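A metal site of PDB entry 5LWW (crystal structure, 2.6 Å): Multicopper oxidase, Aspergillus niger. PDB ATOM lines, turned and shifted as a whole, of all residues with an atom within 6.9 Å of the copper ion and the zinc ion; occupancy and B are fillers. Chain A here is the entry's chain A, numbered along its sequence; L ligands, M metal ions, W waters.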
ATOM      1  N   VAL A 174     -16.067 -13.575  30.655  1.00  0.00           N
ATOM      2  CA  VAL A 174     -15.010 -14.113  29.775  1.00  0.00           C
ATOM      3  C   VAL A 174     -15.544 -14.862  28.533  1.00  0.00           C
ATOM      4  O   VAL A 174     -15.056 -14.626  27.422  1.00  0.00           O
ATOM      5  CB  VAL A 174     -14.018 -14.995  30.533  1.00  0.00           C
ATOM      6  CG1 VAL A 174     -12.999 -15.606  29.569  1.00  0.00           C
ATOM      7  CG2 VAL A 174     -13.324 -14.161  31.593  1.00  0.00           C
ATOM      8  N   GLN A 178     -14.712 -11.668  23.311  1.00  0.00           N
ATOM      9  CA  GLN A 178     -13.586 -12.320  22.660  1.00  0.00           C
ATOM     10  C   GLN A 178     -12.300 -11.749  23.218  1.00  0.00           C
ATOM     11  O   GLN A 178     -11.233 -12.314  23.070  1.00  0.00           O
ATOM     12  CB  GLN A 178     -13.726 -12.256  21.134  1.00  0.00           C
ATOM     13  CG  GLN A 178     -12.506 -12.655  20.343  1.00  0.00           C
ATOM     14  CD  GLN A 178     -12.845 -13.405  19.071  1.00  0.00           C
ATOM     15  OE1 GLN A 178     -13.999 -13.488  18.671  1.00  0.00           O
ATOM     16  NE2 GLN A 178     -11.824 -13.989  18.431  1.00  0.00           N
ATOM     17  N   ASN A 179     -12.429 -10.658  23.963  1.00  0.00           N
ATOM     18  CA  ASN A 179     -11.292 -10.052  24.669  1.00  0.00           C
ATOM     19  C   ASN A 179     -10.885 -10.810  25.927  1.00  0.00           C
ATOM     20  O   ASN A 179     -11.701 -11.466  26.562  1.00  0.00           O
ATOM     21  CB  ASN A 179     -11.574  -8.586  24.985  1.00  0.00           C
ATOM     22  CG  ASN A 179     -12.801  -8.408  25.837  1.00  0.00           C
ATOM     23  OD1 ASN A 179     -12.689  -8.146  27.038  1.00  0.00           O
ATOM     24  ND2 ASN A 179     -13.992  -8.581  25.233  1.00  0.00           N
ATOM     25  N   PRO A 180      -9.595 -10.743  26.278  1.00  0.00           N
ATOM     26  CA  PRO A 180      -9.034 -11.494  27.418  1.00  0.00           C
ATOM     27  C   PRO A 180      -9.606 -11.049  28.735  1.00  0.00           C
ATOM     28  O   PRO A 180     -10.146  -9.950  28.797  1.00  0.00           O
ATOM     29  CB  PRO A 180      -7.547 -11.122  27.390  1.00  0.00           C
ATOM     30  CG  PRO A 180      -7.276 -10.719  26.003  1.00  0.00           C
ATOM     31  CD  PRO A 180      -8.547 -10.164  25.430  1.00  0.00           C
ATOM     32  N   PRO A 181      -9.440 -11.844  29.805  1.00  0.00           N
ATOM     33  CA  PRO A 181      -9.784 -11.405  31.158  1.00  0.00           C
ATOM     34  C   PRO A 181      -8.892 -10.291  31.667  1.00  0.00           C
ATOM     35  O   PRO A 181      -7.695 -10.279  31.328  1.00  0.00           O
ATOM     36  CB  PRO A 181      -9.572 -12.655  32.015  1.00  0.00           C
ATOM     37  CG  PRO A 181      -8.759 -13.566  31.186  1.00  0.00           C
ATOM     38  CD  PRO A 181      -9.040 -13.266  29.758  1.00  0.00           C
ATOM     39  N   HIS A 226      -3.956 -16.278  33.854  1.00  0.00           N
ATOM     40  CA  HIS A 226      -3.907 -15.796  32.489  1.00  0.00           C
ATOM     41  C   HIS A 226      -2.789 -14.816  32.270  1.00  0.00           C
ATOM     42  O   HIS A 226      -2.971 -13.861  31.544  1.00  0.00           O
ATOM     43  CB  HIS A 226      -5.249 -15.164  32.093  1.00  0.00           C
ATOM     44  CG  HIS A 226      -5.529 -15.227  30.623  1.00  0.00           C
ATOM     45  ND1 HIS A 226      -4.669 -14.709  29.678  1.00  0.00           N
ATOM     46  CD2 HIS A 226      -6.585 -15.721  29.935  1.00  0.00           C
ATOM     47  CE1 HIS A 226      -5.191 -14.873  28.469  1.00  0.00           C
ATOM     48  NE2 HIS A 226      -6.354 -15.489  28.602  1.00  0.00           N
ATOM     49  N   CYS A 287       0.137 -11.177  25.997  1.00  0.00           N
ATOM     50  CA  CYS A 287      -0.812 -12.213  26.407  1.00  0.00           C
ATOM     51  C   CYS A 287      -1.248 -12.049  27.901  1.00  0.00           C
ATOM     52  O   CYS A 287      -1.887 -12.948  28.475  1.00  0.00           O
ATOM     53  CB  CYS A 287      -0.191 -13.601  26.140  1.00  0.00           C
ATOM     54  SG  CYS A 287       1.162 -14.058  27.268  1.00  0.00           S
ATOM     55  N   VAL A 352      -5.193 -24.888  16.969  1.00  0.00           N
ATOM     56  CA  VAL A 352      -5.801 -24.135  18.031  1.00  0.00           C
ATOM     57  C   VAL A 352      -6.583 -22.934  17.482  1.00  0.00           C
ATOM     58  O   VAL A 352      -6.022 -22.077  16.796  1.00  0.00           O
ATOM     59  CB  VAL A 352      -4.713 -23.715  19.042  1.00  0.00           C
ATOM     60  CG1 VAL A 352      -5.269 -22.650  19.985  1.00  0.00           C
ATOM     61  CG2 VAL A 352      -4.162 -24.964  19.760  1.00  0.00           C
ATOM     62  N   PHE A 354     -10.351 -20.261  18.161  1.00  0.00           N
ATOM     63  CA  PHE A 354     -11.177 -19.598  19.133  1.00  0.00           C
ATOM     64  C   PHE A 354     -12.462 -19.267  18.397  1.00  0.00           C
ATOM     65  O   PHE A 354     -12.497 -18.293  17.652  1.00  0.00           O
ATOM     66  CB  PHE A 354     -10.436 -18.329  19.570  1.00  0.00           C
ATOM     67  CG  PHE A 354     -11.048 -17.630  20.756  1.00  0.00           C
ATOM     68  CD1 PHE A 354     -11.664 -18.339  21.790  1.00  0.00           C
ATOM     69  CD2 PHE A 354     -11.002 -16.241  20.854  1.00  0.00           C
ATOM     70  CE1 PHE A 354     -12.198 -17.688  22.889  1.00  0.00           C
ATOM     71  CE2 PHE A 354     -11.530 -15.599  21.955  1.00  0.00           C
ATOM     72  CZ  PHE A 354     -12.136 -16.317  22.960  1.00  0.00           C
ATOM     73  N   TRP A 365     -12.325 -22.126  23.136  1.00  0.00           N
ATOM     74  CA  TRP A 365     -11.079 -22.558  22.492  1.00  0.00           C
ATOM     75  C   TRP A 365     -11.223 -23.996  22.087  1.00  0.00           C
ATOM     76  O   TRP A 365     -12.001 -24.734  22.651  1.00  0.00           O
ATOM     77  CB  TRP A 365      -9.883 -22.338  23.389  1.00  0.00           C
ATOM     78  CG  TRP A 365      -9.575 -20.927  23.487  1.00  0.00           C
ATOM     79  CD1 TRP A 365     -10.119 -20.053  24.370  1.00  0.00           C
ATOM     80  CD2 TRP A 365      -8.658 -20.173  22.680  1.00  0.00           C
ATOM     81  NE1 TRP A 365      -9.591 -18.797  24.176  1.00  0.00           N
ATOM     82  CE2 TRP A 365      -8.698 -18.831  23.143  1.00  0.00           C
ATOM     83  CE3 TRP A 365      -7.799 -20.497  21.606  1.00  0.00           C
ATOM     84  CZ2 TRP A 365      -7.910 -17.791  22.565  1.00  0.00           C
ATOM     85  CZ3 TRP A 365      -7.012 -19.457  21.028  1.00  0.00           C
ATOM     86  CH2 TRP A 365      -7.082 -18.129  21.517  1.00  0.00           C
ATOM     87  N   VAL A 419      -2.237 -15.118  19.368  1.00  0.00           N
ATOM     88  CA  VAL A 419      -2.457 -15.495  20.792  1.00  0.00           C
ATOM     89  C   VAL A 419      -1.603 -16.722  21.182  1.00  0.00           C
ATOM     90  O   VAL A 419      -1.834 -17.823  20.684  1.00  0.00           O
ATOM     91  CB  VAL A 419      -3.933 -15.852  21.034  1.00  0.00           C
ATOM     92  CG1 VAL A 419      -4.170 -16.174  22.503  1.00  0.00           C
ATOM     93  CG2 VAL A 419      -4.847 -14.759  20.480  1.00  0.00           C
ATOM     94  N   PRO A 420      -0.639 -16.552  22.085  1.00  0.00           N
ATOM     95  CA  PRO A 420       0.236 -17.667  22.492  1.00  0.00           C
ATOM     96  C   PRO A 420      -0.367 -18.456  23.654  1.00  0.00           C
ATOM     97  O   PRO A 420      -1.219 -17.907  24.374  1.00  0.00           O
ATOM     98  CB  PRO A 420       1.491 -16.938  22.957  1.00  0.00           C
ATOM     99  CG  PRO A 420       0.966 -15.640  23.497  1.00  0.00           C
ATOM    100  CD  PRO A 420      -0.335 -15.311  22.809  1.00  0.00           C
ATOM    101  N   HIS A 421       0.038 -19.731  23.854  1.00  0.00           N
ATOM    102  CA  HIS A 421      -0.539 -20.621  24.943  1.00  0.00           C
ATOM    103  C   HIS A 421       0.464 -21.623  25.568  1.00  0.00           C
ATOM    104  O   HIS A 421       1.090 -22.361  24.853  1.00  0.00           O
ATOM    105  CB  HIS A 421      -1.731 -21.465  24.475  1.00  0.00           C
ATOM    106  CG  HIS A 421      -2.771 -20.710  23.705  1.00  0.00           C
ATOM    107  ND1 HIS A 421      -3.806 -20.043  24.319  1.00  0.00           N
ATOM    108  CD2 HIS A 421      -2.977 -20.563  22.378  1.00  0.00           C
ATOM    109  CE1 HIS A 421      -4.580 -19.488  23.409  1.00  0.00           C
ATOM    110  NE2 HIS A 421      -4.084 -19.783  22.214  1.00  0.00           N
ATOM    111  N   PRO A 422       0.555 -21.687  26.903  1.00  0.00           N
ATOM    112  CA  PRO A 422       1.335 -22.770  27.527  1.00  0.00           C
ATOM    113  C   PRO A 422       0.695 -24.160  27.295  1.00  0.00           C
ATOM    114  O   PRO A 422      -0.500 -24.363  27.462  1.00  0.00           O
ATOM    115  CB  PRO A 422       1.288 -22.388  29.000  1.00  0.00           C
ATOM    116  CG  PRO A 422      -0.064 -21.716  29.149  1.00  0.00           C
ATOM    117  CD  PRO A 422      -0.138 -20.865  27.908  1.00  0.00           C
ATOM    118  N   ILE A 423       1.476 -25.144  26.910  1.00  0.00           N
ATOM    119  CA  ILE A 423       0.922 -26.461  26.566  1.00  0.00           C
ATOM    120  C   ILE A 423       1.625 -27.464  27.488  1.00  0.00           C
ATOM    121  O   ILE A 423       2.862 -27.498  27.634  1.00  0.00           O
ATOM    122  CB  ILE A 423       1.185 -26.804  25.084  1.00  0.00           C
ATOM    123  CG1 ILE A 423       0.653 -25.687  24.122  1.00  0.00           C
ATOM    124  CG2 ILE A 423       0.675 -28.189  24.740  1.00  0.00           C
ATOM    125  CD1 ILE A 423      -0.849 -25.603  23.912  1.00  0.00           C
ATOM    126  N   CYS A 489      -4.007 -26.631  27.208  1.00  0.00           N
ATOM    127  CA  CYS A 489      -3.508 -25.317  27.524  1.00  0.00           C
ATOM    128  C   CYS A 489      -3.598 -25.114  29.020  1.00  0.00           C
ATOM    129  O   CYS A 489      -4.658 -25.368  29.626  1.00  0.00           O
ATOM    130  CB  CYS A 489      -4.339 -24.267  26.812  1.00  0.00           C
ATOM    131  SG  CYS A 489      -3.754 -22.658  27.309  1.00  0.00           S
ATOM    132  N   HIS A 490      -2.489 -24.684  29.618  1.00  0.00           N
ATOM    133  CA  HIS A 490      -2.452 -24.517  31.054  1.00  0.00           C
ATOM    134  C   HIS A 490      -3.142 -23.248  31.530  1.00  0.00           C
ATOM    135  O   HIS A 490      -3.191 -22.978  32.735  1.00  0.00           O
ATOM    136  CB  HIS A 490      -1.039 -24.626  31.627  1.00  0.00           C
ATOM    137  CG  HIS A 490      -1.025 -25.142  33.044  1.00  0.00           C
ATOM    138  ND1 HIS A 490      -1.336 -24.353  34.131  1.00  0.00           N
ATOM    139  CD2 HIS A 490      -0.776 -26.377  33.532  1.00  0.00           C
ATOM    140  CE1 HIS A 490      -1.277 -25.080  35.231  1.00  0.00           C
ATOM    141  NE2 HIS A 490      -0.934 -26.320  34.892  1.00  0.00           N
ATOM    142  N   ILE A 491      -3.710 -22.470  30.600  1.00  0.00           N
ATOM    143  CA  ILE A 491      -4.575 -21.352  30.964  1.00  0.00           C
ATOM    144  C   ILE A 491      -5.941 -21.910  31.467  1.00  0.00           C
ATOM    145  O   ILE A 491      -6.624 -22.639  30.738  1.00  0.00           O
ATOM    146  CB  ILE A 491      -4.742 -20.355  29.813  1.00  0.00           C
ATOM    147  CG1 ILE A 491      -3.423 -19.645  29.569  1.00  0.00           C
ATOM    148  CG2 ILE A 491      -5.865 -19.384  30.124  1.00  0.00           C
ATOM    149  CD1 ILE A 491      -3.322 -18.834  28.286  1.00  0.00           C
ATOM    150  N   GLY A 492      -6.300 -21.593  32.702  1.00  0.00           N
ATOM    151  CA  GLY A 492      -7.536 -22.076  33.313  1.00  0.00           C
ATOM    152  C   GLY A 492      -8.777 -22.010  32.445  1.00  0.00           C
ATOM    153  O   GLY A 492      -9.348 -23.062  32.115  1.00  0.00           O
ATOM    154  N   PHE A 493      -9.186 -20.788  32.065  1.00  0.00           N
ATOM    155  CA  PHE A 493     -10.381 -20.544  31.246  1.00  0.00           C
ATOM    156  C   PHE A 493     -10.330 -21.286  29.894  1.00  0.00           C
ATOM    157  O   PHE A 493     -11.340 -21.859  29.440  1.00  0.00           O
ATOM    158  CB  PHE A 493     -10.590 -19.038  30.964  1.00  0.00           C
ATOM    159  CG  PHE A 493     -10.819 -18.178  32.182  1.00  0.00           C
ATOM    160  CD1 PHE A 493     -11.977 -18.336  32.971  1.00  0.00           C
ATOM    161  CD2 PHE A 493      -9.916 -17.157  32.505  1.00  0.00           C
ATOM    162  CE1 PHE A 493     -12.198 -17.523  34.080  1.00  0.00           C
ATOM    163  CE2 PHE A 493     -10.136 -16.344  33.605  1.00  0.00           C
ATOM    164  CZ  PHE A 493     -11.268 -16.522  34.388  1.00  0.00           C
ATOM    165  N   HIS A 494      -9.182 -21.284  29.223  1.00  0.00           N
ATOM    166  CA  HIS A 494      -9.086 -21.985  27.956  1.00  0.00           C
ATOM    167  C   HIS A 494      -9.385 -23.474  28.096  1.00  0.00           C
ATOM    168  O   HIS A 494     -10.146 -24.013  27.295  1.00  0.00           O
ATOM    169  CB  HIS A 494      -7.733 -21.775  27.256  1.00  0.00           C
ATOM    170  CG  HIS A 494      -7.384 -20.328  27.024  1.00  0.00           C
ATOM    171  ND1 HIS A 494      -6.168 -19.925  26.516  1.00  0.00           N
ATOM    172  CD2 HIS A 494      -8.081 -19.191  27.282  1.00  0.00           C
ATOM    173  CE1 HIS A 494      -6.157 -18.611  26.420  1.00  0.00           C
ATOM    174  NE2 HIS A 494      -7.295 -18.148  26.896  1.00  0.00           N
ATOM    175  N   ALA A 495      -8.818 -24.134  29.101  1.00  0.00           N
ATOM    176  CA  ALA A 495      -9.011 -25.588  29.267  1.00  0.00           C
ATOM    177  C   ALA A 495     -10.454 -25.907  29.623  1.00  0.00           C
ATOM    178  O   ALA A 495     -10.983 -26.940  29.238  1.00  0.00           O
ATOM    179  CB  ALA A 495      -8.065 -26.122  30.314  1.00  0.00           C
ATOM    180  N   GLU A 497     -12.956 -24.252  28.598  1.00  0.00           N
ATOM    181  CA  GLU A 497     -13.742 -23.959  27.415  1.00  0.00           C
ATOM    182  C   GLU A 497     -13.507 -25.021  26.341  1.00  0.00           C
ATOM    183  O   GLU A 497     -14.116 -24.990  25.291  1.00  0.00           O
ATOM    184  CB  GLU A 497     -13.383 -22.584  26.905  1.00  0.00           C
ATOM    185  CG  GLU A 497     -13.910 -21.453  27.758  1.00  0.00           C
ATOM    186  CD  GLU A 497     -13.285 -20.098  27.422  1.00  0.00           C
ATOM    187  OE1 GLU A 497     -12.350 -20.051  26.594  1.00  0.00           O
ATOM    188  OE2 GLU A 497     -13.725 -19.085  28.000  1.00  0.00           O
ATOM    189  N   PHE A 499     -10.099 -26.293  25.401  1.00  0.00           N
ATOM    190  CA  PHE A 499      -8.684 -26.311  24.905  1.00  0.00           C
ATOM    191  C   PHE A 499      -7.854 -27.411  25.599  1.00  0.00           C
ATOM    192  O   PHE A 499      -6.982 -27.149  26.473  1.00  0.00           O
ATOM    193  CB  PHE A 499      -8.010 -24.922  25.062  1.00  0.00           C
ATOM    194  CG  PHE A 499      -6.716 -24.758  24.304  1.00  0.00           C
ATOM    195  CD1 PHE A 499      -5.909 -25.833  23.990  1.00  0.00           C
ATOM    196  CD2 PHE A 499      -6.278 -23.499  23.954  1.00  0.00           C
ATOM    197  CE1 PHE A 499      -4.702 -25.678  23.300  1.00  0.00           C
ATOM    198  CE2 PHE A 499      -5.062 -23.324  23.275  1.00  0.00           C
ATOM    199  CZ  PHE A 499      -4.271 -24.425  22.939  1.00  0.00           C
HETATM  200 CL1  LIG L   1      -7.774 -14.443  24.939  1.00  0.00          CL
HETATM  201 CU    CU M   1      -4.599 -21.048  26.100  1.00  0.00          CU
HETATM  202 ZN    ZN M   2      -7.783 -16.135  27.274  1.00  0.00          ZN
HETATM  203  O   HOH W   1      -9.560 -16.258  28.430  1.00  0.00           O
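The backbone NH of Ile 491 sits close to the side-chain sulfur of Cys 489.
NE2 of His 421 is in hydrogen-bond range of O of Val 419, 3.4 Å away.
The side-chain sulfur (SG) of Cys 489 sits close to the backbone carbonyl oxygen (O) of Pro 422 (3.7 Å).
N of Cys 489 lies within hydrogen-bond range of O of Phe 499 (3.1 Å).
N of Phe 499 is in hydrogen-bond range of O of His 494 (3.0 Å).
Residues that only touch the copper ion: Ile 491 and Phe 499.
Pro 181 touches the zinc ion (CD to ZN, 3.998 Å).
Within 4 Å of the zinc ion: Pro 181, His 226 and His 494.
The copper ion is bound by ND1 of His 494 (2.0 Å), SG of Cys 489 (2.2 Å) and ND1 of His 421 (2.2 Å).
The copper ion has three donor atoms within binding distance.
NE2 of His 226 binds the zinc ion (2.1 Å).
NE2 of His 494 is bound to the zinc ion (2.1 Å).
The zinc ion is bound by water W1 (2.1 Å).
The zinc ion has three donor atoms within binding distance.
Slightly farther from the zinc ion lies a chlorine (CL1) of the ligand (2.9 Å).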
